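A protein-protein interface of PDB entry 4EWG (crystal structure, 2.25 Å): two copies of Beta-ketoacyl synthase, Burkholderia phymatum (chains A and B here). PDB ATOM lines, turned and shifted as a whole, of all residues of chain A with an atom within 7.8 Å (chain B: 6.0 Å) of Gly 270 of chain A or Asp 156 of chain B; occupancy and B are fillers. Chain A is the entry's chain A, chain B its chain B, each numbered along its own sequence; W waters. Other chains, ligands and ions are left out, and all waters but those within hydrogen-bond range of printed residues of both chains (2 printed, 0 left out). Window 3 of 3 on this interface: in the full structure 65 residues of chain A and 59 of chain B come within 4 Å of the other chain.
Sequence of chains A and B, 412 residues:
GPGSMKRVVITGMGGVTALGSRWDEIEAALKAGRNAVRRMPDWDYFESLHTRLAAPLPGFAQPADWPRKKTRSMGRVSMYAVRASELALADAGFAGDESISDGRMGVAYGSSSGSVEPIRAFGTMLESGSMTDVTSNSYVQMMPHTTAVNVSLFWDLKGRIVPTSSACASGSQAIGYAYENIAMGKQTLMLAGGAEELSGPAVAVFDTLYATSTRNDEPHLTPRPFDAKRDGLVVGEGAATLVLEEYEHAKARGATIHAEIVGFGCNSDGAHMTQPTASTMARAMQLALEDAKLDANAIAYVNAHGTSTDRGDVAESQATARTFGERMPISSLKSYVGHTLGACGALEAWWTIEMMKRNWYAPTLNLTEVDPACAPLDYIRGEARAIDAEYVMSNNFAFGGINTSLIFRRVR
The backbone carbonyl oxygen (O) of Lys 158 of chain B sits at hydrogen-bond distance from the backbone NH (N) of Ser 268 of chain A (3.2 Å).
The side-chain carboxylate (OD2) of Asp 156 of chain B lies close to the backbone carbonyl oxygen (O) of Gly 270 of chain A (3.0 Å).
ND2 of Asn 403 of chain A sits at hydrogen-bond distance from OD1 of Asp 269 of chain A (3.0 Å).
OD2 of Asp 269 of chain A sits at hydrogen-bond distance from N of Thr 277 of chain A, 2.9 Å away.
N of Asp 269 of chain A is in hydrogen-bond range of O of Gly 401 of chain A.
OD1 of Asp 269 of chain A sits at hydrogen-bond distance from OG1 of Thr 280 of chain A.
O of Asn 267 of chain A sits at hydrogen-bond distance from N of Asn 403 of chain A, at 2.8 Å.
O of Ser 152 of chain B lies within hydrogen-bond range of N of Leu 157 of chain B (2.9 Å).
CB of Asn 267 of chain A touches O of Lys 158 of chain B (3.4 Å).
OG of Ser 268 of chain A touches O of Leu 157 of chain B, at 3.9 Å.
Asp 269 of chain A touches Lys 158 of chain B.
Gly 270 of chain A touches Leu 153 of chain B.
CA of Gly 270 of chain A touches O of Leu 157 of chain B (3.1 Å).
N of Gly 270 of chain A touches CG of Lys 158 of chain B, at 3.99 Å.
Leu 153 of chain B touches Ala 271 of chain A.
CE of Met 273 of chain A touches CD1 of Leu 153 of chain B, at 3.1 Å.
Asp 156 of chain B touches one residue of chain A.
Of the printed residues of chain B, Ser 268 of chain A touches Leu 157 (3.9 Å) and Lys 158 (3.2 Å).
Printed residues of chain A within 4 Å of Leu 157 of chain B: Ser 268 and Gly 270.
Thr 277 of chain A touches none of the printed residues of chain B.
Gly 401 of chain A touches none of the printed residues of chain B.
The nearest residue of chain A that does not touch Asp 156 of chain B is Ala 271 of chain A (4.6 Å).
Of the 13 printed residues of chain A, 6 touch a printed residue of chain B.
Hydrophobic or aromatic side chains of chain A that line the printed part of chain B: Met 273.
Hydrophobic or aromatic side chains of chain B within 4 Å of the printed part of chain A: Leu 153.
Among the printed residues, no Asp or Glu carboxylate lies within 4 Å of a Lys or Arg side-chain nitrogen of the other chain.
No position is printed for both chains.
Of the 10 pairs that touch across the chains among the printed residues, none has its exchanged pair printed and touching as well.
Water W1 lies within hydrogen-bond range of O of Leu 157 of chain B (2.4 Å), OG of Ser 152 of chain B (2.6 Å) and OG of Ser 268 of chain A (3.2 Å).
Water W2 bridges the side-chain amide nitrogen (ND2) of Asn 267 of chain A and the backbone carbonyl oxygen (O) of Lys 158 of chain B.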
ATOM      1  N   ASN A 267      -9.608  31.339 -10.650  1.00  0.00           N
ATOM      2  CA  ASN A 267     -10.145  30.128 -11.246  1.00  0.00           C
ATOM      3  C   ASN A 267     -10.203  30.237 -12.770  1.00  0.00           C
ATOM      4  O   ASN A 267      -9.682  31.182 -13.333  1.00  0.00           O
ATOM      5  CB  ASN A 267     -11.529  29.776 -10.648  1.00  0.00           C
ATOM      6  CG  ASN A 267     -12.634  30.703 -11.103  1.00  0.00           C
ATOM      7  OD1 ASN A 267     -12.386  31.745 -11.707  1.00  0.00           O
ATOM      8  ND2 ASN A 267     -13.870  30.320 -10.821  1.00  0.00           N
ATOM      9  N   SER A 268     -10.783  29.235 -13.420  1.00  0.00           N
ATOM     10  CA  SER A 268     -11.106  29.340 -14.846  1.00  0.00           C
ATOM     11  C   SER A 268     -12.478  28.779 -15.205  1.00  0.00           C
ATOM     12  O   SER A 268     -13.058  27.950 -14.485  1.00  0.00           O
ATOM     13  CB  SER A 268     -10.035  28.722 -15.727  1.00  0.00           C
ATOM     14  OG  SER A 268      -9.468  27.638 -15.079  1.00  0.00           O
ATOM     15  N   ASP A 269     -12.986  29.259 -16.336  1.00  0.00           N
ATOM     16  CA  ASP A 269     -14.295  28.854 -16.838  1.00  0.00           C
ATOM     17  C   ASP A 269     -14.333  27.398 -17.299  1.00  0.00           C
ATOM     18  O   ASP A 269     -15.382  26.785 -17.276  1.00  0.00           O
ATOM     19  CB  ASP A 269     -14.720  29.728 -18.019  1.00  0.00           C
ATOM     20  CG  ASP A 269     -14.898  31.215 -17.658  1.00  0.00           C
ATOM     21  OD1 ASP A 269     -15.082  31.534 -16.453  1.00  0.00           O
ATOM     22  OD2 ASP A 269     -14.882  32.055 -18.614  1.00  0.00           O
ATOM     23  N   GLY A 270     -13.196  26.871 -17.742  1.00  0.00           N
ATOM     24  CA  GLY A 270     -13.108  25.553 -18.314  1.00  0.00           C
ATOM     25  C   GLY A 270     -14.128  25.247 -19.413  1.00  0.00           C
ATOM     26  O   GLY A 270     -14.632  24.117 -19.497  1.00  0.00           O
ATOM     27  N   ALA A 271     -14.442  26.237 -20.243  1.00  0.00           N
ATOM     28  CA  ALA A 271     -15.512  26.126 -21.202  1.00  0.00           C
ATOM     29  C   ALA A 271     -14.990  26.562 -22.530  1.00  0.00           C
ATOM     30  O   ALA A 271     -14.928  25.773 -23.439  1.00  0.00           O
ATOM     31  CB  ALA A 271     -16.727  26.973 -20.783  1.00  0.00           C
ATOM     32  N   HIS A 272     -14.638  27.831 -22.655  1.00  0.00           N
ATOM     33  CA  HIS A 272     -14.191  28.393 -23.937  1.00  0.00           C
ATOM     34  C   HIS A 272     -12.894  29.176 -23.830  1.00  0.00           C
ATOM     35  O   HIS A 272     -12.528  29.717 -22.747  1.00  0.00           O
ATOM     36  CB  HIS A 272     -15.286  29.285 -24.503  1.00  0.00           C
ATOM     37  CG  HIS A 272     -15.229  29.438 -26.002  1.00  0.00           C
ATOM     38  ND1 HIS A 272     -14.484  30.402 -26.620  1.00  0.00           N
ATOM     39  CD2 HIS A 272     -15.838  28.703 -27.021  1.00  0.00           C
ATOM     40  CE1 HIS A 272     -14.632  30.290 -27.949  1.00  0.00           C
ATOM     41  NE2 HIS A 272     -15.459  29.249 -28.194  1.00  0.00           N
ATOM     42  N   MET A 273     -12.190  29.244 -24.962  1.00  0.00           N
ATOM     43  CA  MET A 273     -10.924  29.963 -25.047  1.00  0.00           C
ATOM     44  C   MET A 273     -11.109  31.504 -24.987  1.00  0.00           C
ATOM     45  O   MET A 273     -10.266  32.216 -24.434  1.00  0.00           O
ATOM     46  CB  MET A 273     -10.190  29.585 -26.335  1.00  0.00           C
ATOM     47  CG  MET A 273      -8.771  30.122 -26.415  1.00  0.00           C
ATOM     48  SD  MET A 273      -7.677  29.401 -25.151  1.00  0.00           S
ATOM     49  CE  MET A 273      -7.712  27.660 -25.729  1.00  0.00           C
ATOM     50  N   THR A 277     -17.649  32.733 -19.368  1.00  0.00           N
ATOM     51  CA  THR A 277     -18.804  32.149 -18.680  1.00  0.00           C
ATOM     52  C   THR A 277     -19.075  32.846 -17.318  1.00  0.00           C
ATOM     53  O   THR A 277     -18.284  32.734 -16.358  1.00  0.00           O
ATOM     54  CB  THR A 277     -18.585  30.645 -18.395  1.00  0.00           C
ATOM     55  OG1 THR A 277     -18.263  29.965 -19.612  1.00  0.00           O
ATOM     56  CG2 THR A 277     -19.859  30.031 -17.773  1.00  0.00           C
ATOM     57  N   THR A 280     -18.622  31.097 -13.453  1.00  0.00           N
ATOM     58  CA  THR A 280     -17.267  30.904 -12.959  1.00  0.00           C
ATOM     59  C   THR A 280     -16.539  32.221 -12.739  1.00  0.00           C
ATOM     60  O   THR A 280     -15.660  32.289 -11.878  1.00  0.00           O
ATOM     61  CB  THR A 280     -16.452  29.960 -13.866  1.00  0.00           C
ATOM     62  OG1 THR A 280     -16.867  30.149 -15.223  1.00  0.00           O
ATOM     63  CG2 THR A 280     -16.708  28.491 -13.479  1.00  0.00           C
ATOM     64  N   GLY A 400      -8.456  32.135 -22.329  1.00  0.00           N
ATOM     65  CA  GLY A 400      -8.536  30.833 -21.710  1.00  0.00           C
ATOM     66  C   GLY A 400      -9.516  30.766 -20.536  1.00  0.00           C
ATOM     67  O   GLY A 400      -9.558  29.770 -19.821  1.00  0.00           O
ATOM     68  N   GLY A 401     -10.297  31.812 -20.327  1.00  0.00           N
ATOM     69  CA  GLY A 401     -11.248  31.820 -19.234  1.00  0.00           C
ATOM     70  C   GLY A 401     -10.605  31.955 -17.861  1.00  0.00           C
ATOM     71  O   GLY A 401     -11.220  31.557 -16.870  1.00  0.00           O
ATOM     72  N   ILE A 402      -9.376  32.498 -17.801  1.00  0.00           N
ATOM     73  CA  ILE A 402      -8.667  32.708 -16.530  1.00  0.00           C
ATOM     74  C   ILE A 402      -9.257  33.914 -15.824  1.00  0.00           C
ATOM     75  O   ILE A 402      -9.231  35.039 -16.373  1.00  0.00           O
ATOM     76  CB  ILE A 402      -7.156  32.950 -16.738  1.00  0.00           C
ATOM     77  CG1 ILE A 402      -6.485  31.668 -17.252  1.00  0.00           C
ATOM     78  CG2 ILE A 402      -6.488  33.421 -15.461  1.00  0.00           C
ATOM     79  CD1 ILE A 402      -5.088  31.884 -17.828  1.00  0.00           C
ATOM     80  N   ASN A 403      -9.782  33.690 -14.610  1.00  0.00           N
ATOM     81  CA  ASN A 403     -10.392  34.747 -13.832  1.00  0.00           C
ATOM     82  C   ASN A 403      -9.615  35.058 -12.546  1.00  0.00           C
ATOM     83  O   ASN A 403      -9.156  34.140 -11.849  1.00  0.00           O
ATOM     84  CB  ASN A 403     -11.822  34.362 -13.465  1.00  0.00           C
ATOM     85  CG  ASN A 403     -12.589  33.792 -14.643  1.00  0.00           C
ATOM     86  OD1 ASN A 403     -12.564  34.355 -15.748  1.00  0.00           O
ATOM     87  ND2 ASN A 403     -13.256  32.678 -14.420  1.00  0.00           N
ATOM     88  N   SER B 101     -13.168  18.230 -12.790  1.00  0.00           N
ATOM     89  CA  SER B 101     -13.396  19.488 -13.470  1.00  0.00           C
ATOM     90  C   SER B 101     -14.219  20.501 -12.639  1.00  0.00           C
ATOM     91  O   SER B 101     -14.622  21.519 -13.150  1.00  0.00           O
ATOM     92  CB  SER B 101     -14.068  19.217 -14.806  1.00  0.00           C
ATOM     93  OG  SER B 101     -15.348  18.762 -14.577  1.00  0.00           O
ATOM     94  N   ASP B 102     -14.478  20.213 -11.370  1.00  0.00           N
ATOM     95  CA  ASP B 102     -15.403  21.012 -10.594  1.00  0.00           C
ATOM     96  C   ASP B 102     -14.747  22.197  -9.922  1.00  0.00           C
ATOM     97  O   ASP B 102     -15.346  22.780  -9.026  1.00  0.00           O
ATOM     98  CB  ASP B 102     -16.091  20.153  -9.513  1.00  0.00           C
ATOM     99  CG  ASP B 102     -15.188  19.866  -8.291  1.00  0.00           C
ATOM    100  OD1 ASP B 102     -14.014  20.265  -8.249  1.00  0.00           O
ATOM    101  OD2 ASP B 102     -15.682  19.248  -7.353  1.00  0.00           O
ATOM    102  N   VAL B 151      -3.979  22.269 -21.644  1.00  0.00           N
ATOM    103  CA  VAL B 151      -4.165  21.158 -20.761  1.00  0.00           C
ATOM    104  C   VAL B 151      -5.419  21.351 -19.928  1.00  0.00           C
ATOM    105  O   VAL B 151      -6.271  20.479 -19.856  1.00  0.00           O
ATOM    106  CB  VAL B 151      -2.947  20.980 -19.815  1.00  0.00           C
ATOM    107  CG1 VAL B 151      -3.241  19.929 -18.739  1.00  0.00           C
ATOM    108  CG2 VAL B 151      -1.709  20.591 -20.597  1.00  0.00           C
ATOM    109  N   SER B 152      -5.552  22.522 -19.317  1.00  0.00           N
ATOM    110  CA  SER B 152      -6.722  22.814 -18.472  1.00  0.00           C
ATOM    111  C   SER B 152      -8.044  22.741 -19.238  1.00  0.00           C
ATOM    112  O   SER B 152      -8.996  22.157 -18.771  1.00  0.00           O
ATOM    113  CB  SER B 152      -6.613  24.205 -17.858  1.00  0.00           C
ATOM    114  OG  SER B 152      -7.658  24.419 -16.922  1.00  0.00           O
ATOM    115  N   LEU B 153      -8.100  23.419 -20.373  1.00  0.00           N
ATOM    116  CA  LEU B 153      -9.290  23.421 -21.202  1.00  0.00           C
ATOM    117  C   LEU B 153      -9.653  22.019 -21.667  1.00  0.00           C
ATOM    118  O   LEU B 153     -10.810  21.709 -21.798  1.00  0.00           O
ATOM    119  CB  LEU B 153      -9.108  24.295 -22.432  1.00  0.00           C
ATOM    120  CG  LEU B 153      -9.515  25.739 -22.172  1.00  0.00           C
ATOM    121  CD1 LEU B 153      -9.495  26.541 -23.469  1.00  0.00           C
ATOM    122  CD2 LEU B 153     -10.910  25.816 -21.550  1.00  0.00           C
ATOM    123  N   PHE B 154      -8.657  21.195 -21.932  1.00  0.00           N
ATOM    124  CA  PHE B 154      -8.904  19.893 -22.514  1.00  0.00           C
ATOM    125  C   PHE B 154      -9.792  19.029 -21.613  1.00  0.00           C
ATOM    126  O   PHE B 154     -10.617  18.254 -22.116  1.00  0.00           O
ATOM    127  CB  PHE B 154      -7.589  19.188 -22.794  1.00  0.00           C
ATOM    128  CG  PHE B 154      -7.710  18.066 -23.780  1.00  0.00           C
ATOM    129  CD1 PHE B 154      -7.739  18.346 -25.167  1.00  0.00           C
ATOM    130  CD2 PHE B 154      -7.810  16.761 -23.354  1.00  0.00           C
ATOM    131  CE1 PHE B 154      -7.858  17.337 -26.073  1.00  0.00           C
ATOM    132  CE2 PHE B 154      -7.921  15.742 -24.264  1.00  0.00           C
ATOM    133  CZ  PHE B 154      -7.947  16.023 -25.630  1.00  0.00           C
ATOM    134  N   TRP B 155      -9.650  19.159 -20.289  1.00  0.00           N
ATOM    135  CA  TRP B 155     -10.539  18.414 -19.362  1.00  0.00           C
ATOM    136  C   TRP B 155     -11.538  19.301 -18.688  1.00  0.00           C
ATOM    137  O   TRP B 155     -12.099  18.955 -17.660  1.00  0.00           O
ATOM    138  CB  TRP B 155      -9.717  17.642 -18.337  1.00  0.00           C
ATOM    139  CG  TRP B 155      -9.050  16.455 -18.958  1.00  0.00           C
ATOM    140  CD1 TRP B 155      -9.571  15.193 -19.098  1.00  0.00           C
ATOM    141  CD2 TRP B 155      -7.730  16.393 -19.557  1.00  0.00           C
ATOM    142  NE1 TRP B 155      -8.686  14.378 -19.729  1.00  0.00           N
ATOM    143  CE2 TRP B 155      -7.552  15.033 -20.005  1.00  0.00           C
ATOM    144  CE3 TRP B 155      -6.710  17.289 -19.743  1.00  0.00           C
ATOM    145  CZ2 TRP B 155      -6.408  14.614 -20.653  1.00  0.00           C
ATOM    146  CZ3 TRP B 155      -5.553  16.866 -20.370  1.00  0.00           C
ATOM    147  CH2 TRP B 155      -5.411  15.553 -20.822  1.00  0.00           C
ATOM    148  N   ASP B 156     -11.776  20.456 -19.278  1.00  0.00           N
ATOM    149  CA  ASP B 156     -12.742  21.385 -18.768  1.00  0.00           C
ATOM    150  C   ASP B 156     -12.533  21.695 -17.306  1.00  0.00           C
ATOM    151  O   ASP B 156     -13.470  21.869 -16.557  1.00  0.00           O
ATOM    152  CB  ASP B 156     -14.119  20.862 -19.052  1.00  0.00           C
ATOM    153  CG  ASP B 156     -14.468  21.033 -20.465  1.00  0.00           C
ATOM    154  OD1 ASP B 156     -13.647  20.711 -21.332  1.00  0.00           O
ATOM    155  OD2 ASP B 156     -15.544  21.554 -20.749  1.00  0.00           O
ATOM    156  N   LEU B 157     -11.264  21.779 -16.924  1.00  0.00           N
ATOM    157  CA  LEU B 157     -10.906  22.032 -15.542  1.00  0.00           C
ATOM    158  C   LEU B 157     -11.230  23.496 -15.221  1.00  0.00           C
ATOM    159  O   LEU B 157     -11.231  24.344 -16.108  1.00  0.00           O
ATOM    160  CB  LEU B 157      -9.425  21.737 -15.291  1.00  0.00           C
ATOM    161  CG  LEU B 157      -8.937  20.335 -15.656  1.00  0.00           C
ATOM    162  CD1 LEU B 157      -7.412  20.291 -15.557  1.00  0.00           C
ATOM    163  CD2 LEU B 157      -9.618  19.295 -14.752  1.00  0.00           C
ATOM    164  N   LYS B 158     -11.531  23.773 -13.958  1.00  0.00           N
ATOM    165  CA  LYS B 158     -11.983  25.091 -13.570  1.00  0.00           C
ATOM    166  C   LYS B 158     -11.181  25.635 -12.380  1.00  0.00           C
ATOM    167  O   LYS B 158     -11.591  26.592 -11.736  1.00  0.00           O
ATOM    168  CB  LYS B 158     -13.509  25.053 -13.293  1.00  0.00           C
ATOM    169  CG  LYS B 158     -14.358  24.771 -14.559  1.00  0.00           C
ATOM    170  CD  LYS B 158     -15.824  24.406 -14.289  1.00  0.00           C
ATOM    171  CE  LYS B 158     -16.447  23.713 -15.511  1.00  0.00           C
ATOM    172  NZ  LYS B 158     -15.975  22.310 -15.648  1.00  0.00           N
HETATM  173  O   HOH W   1      -9.797  25.661 -17.583  1.00  0.00           O
HETATM  174  O   HOH W   2     -13.958  27.597 -10.090  1.00  0.00           O
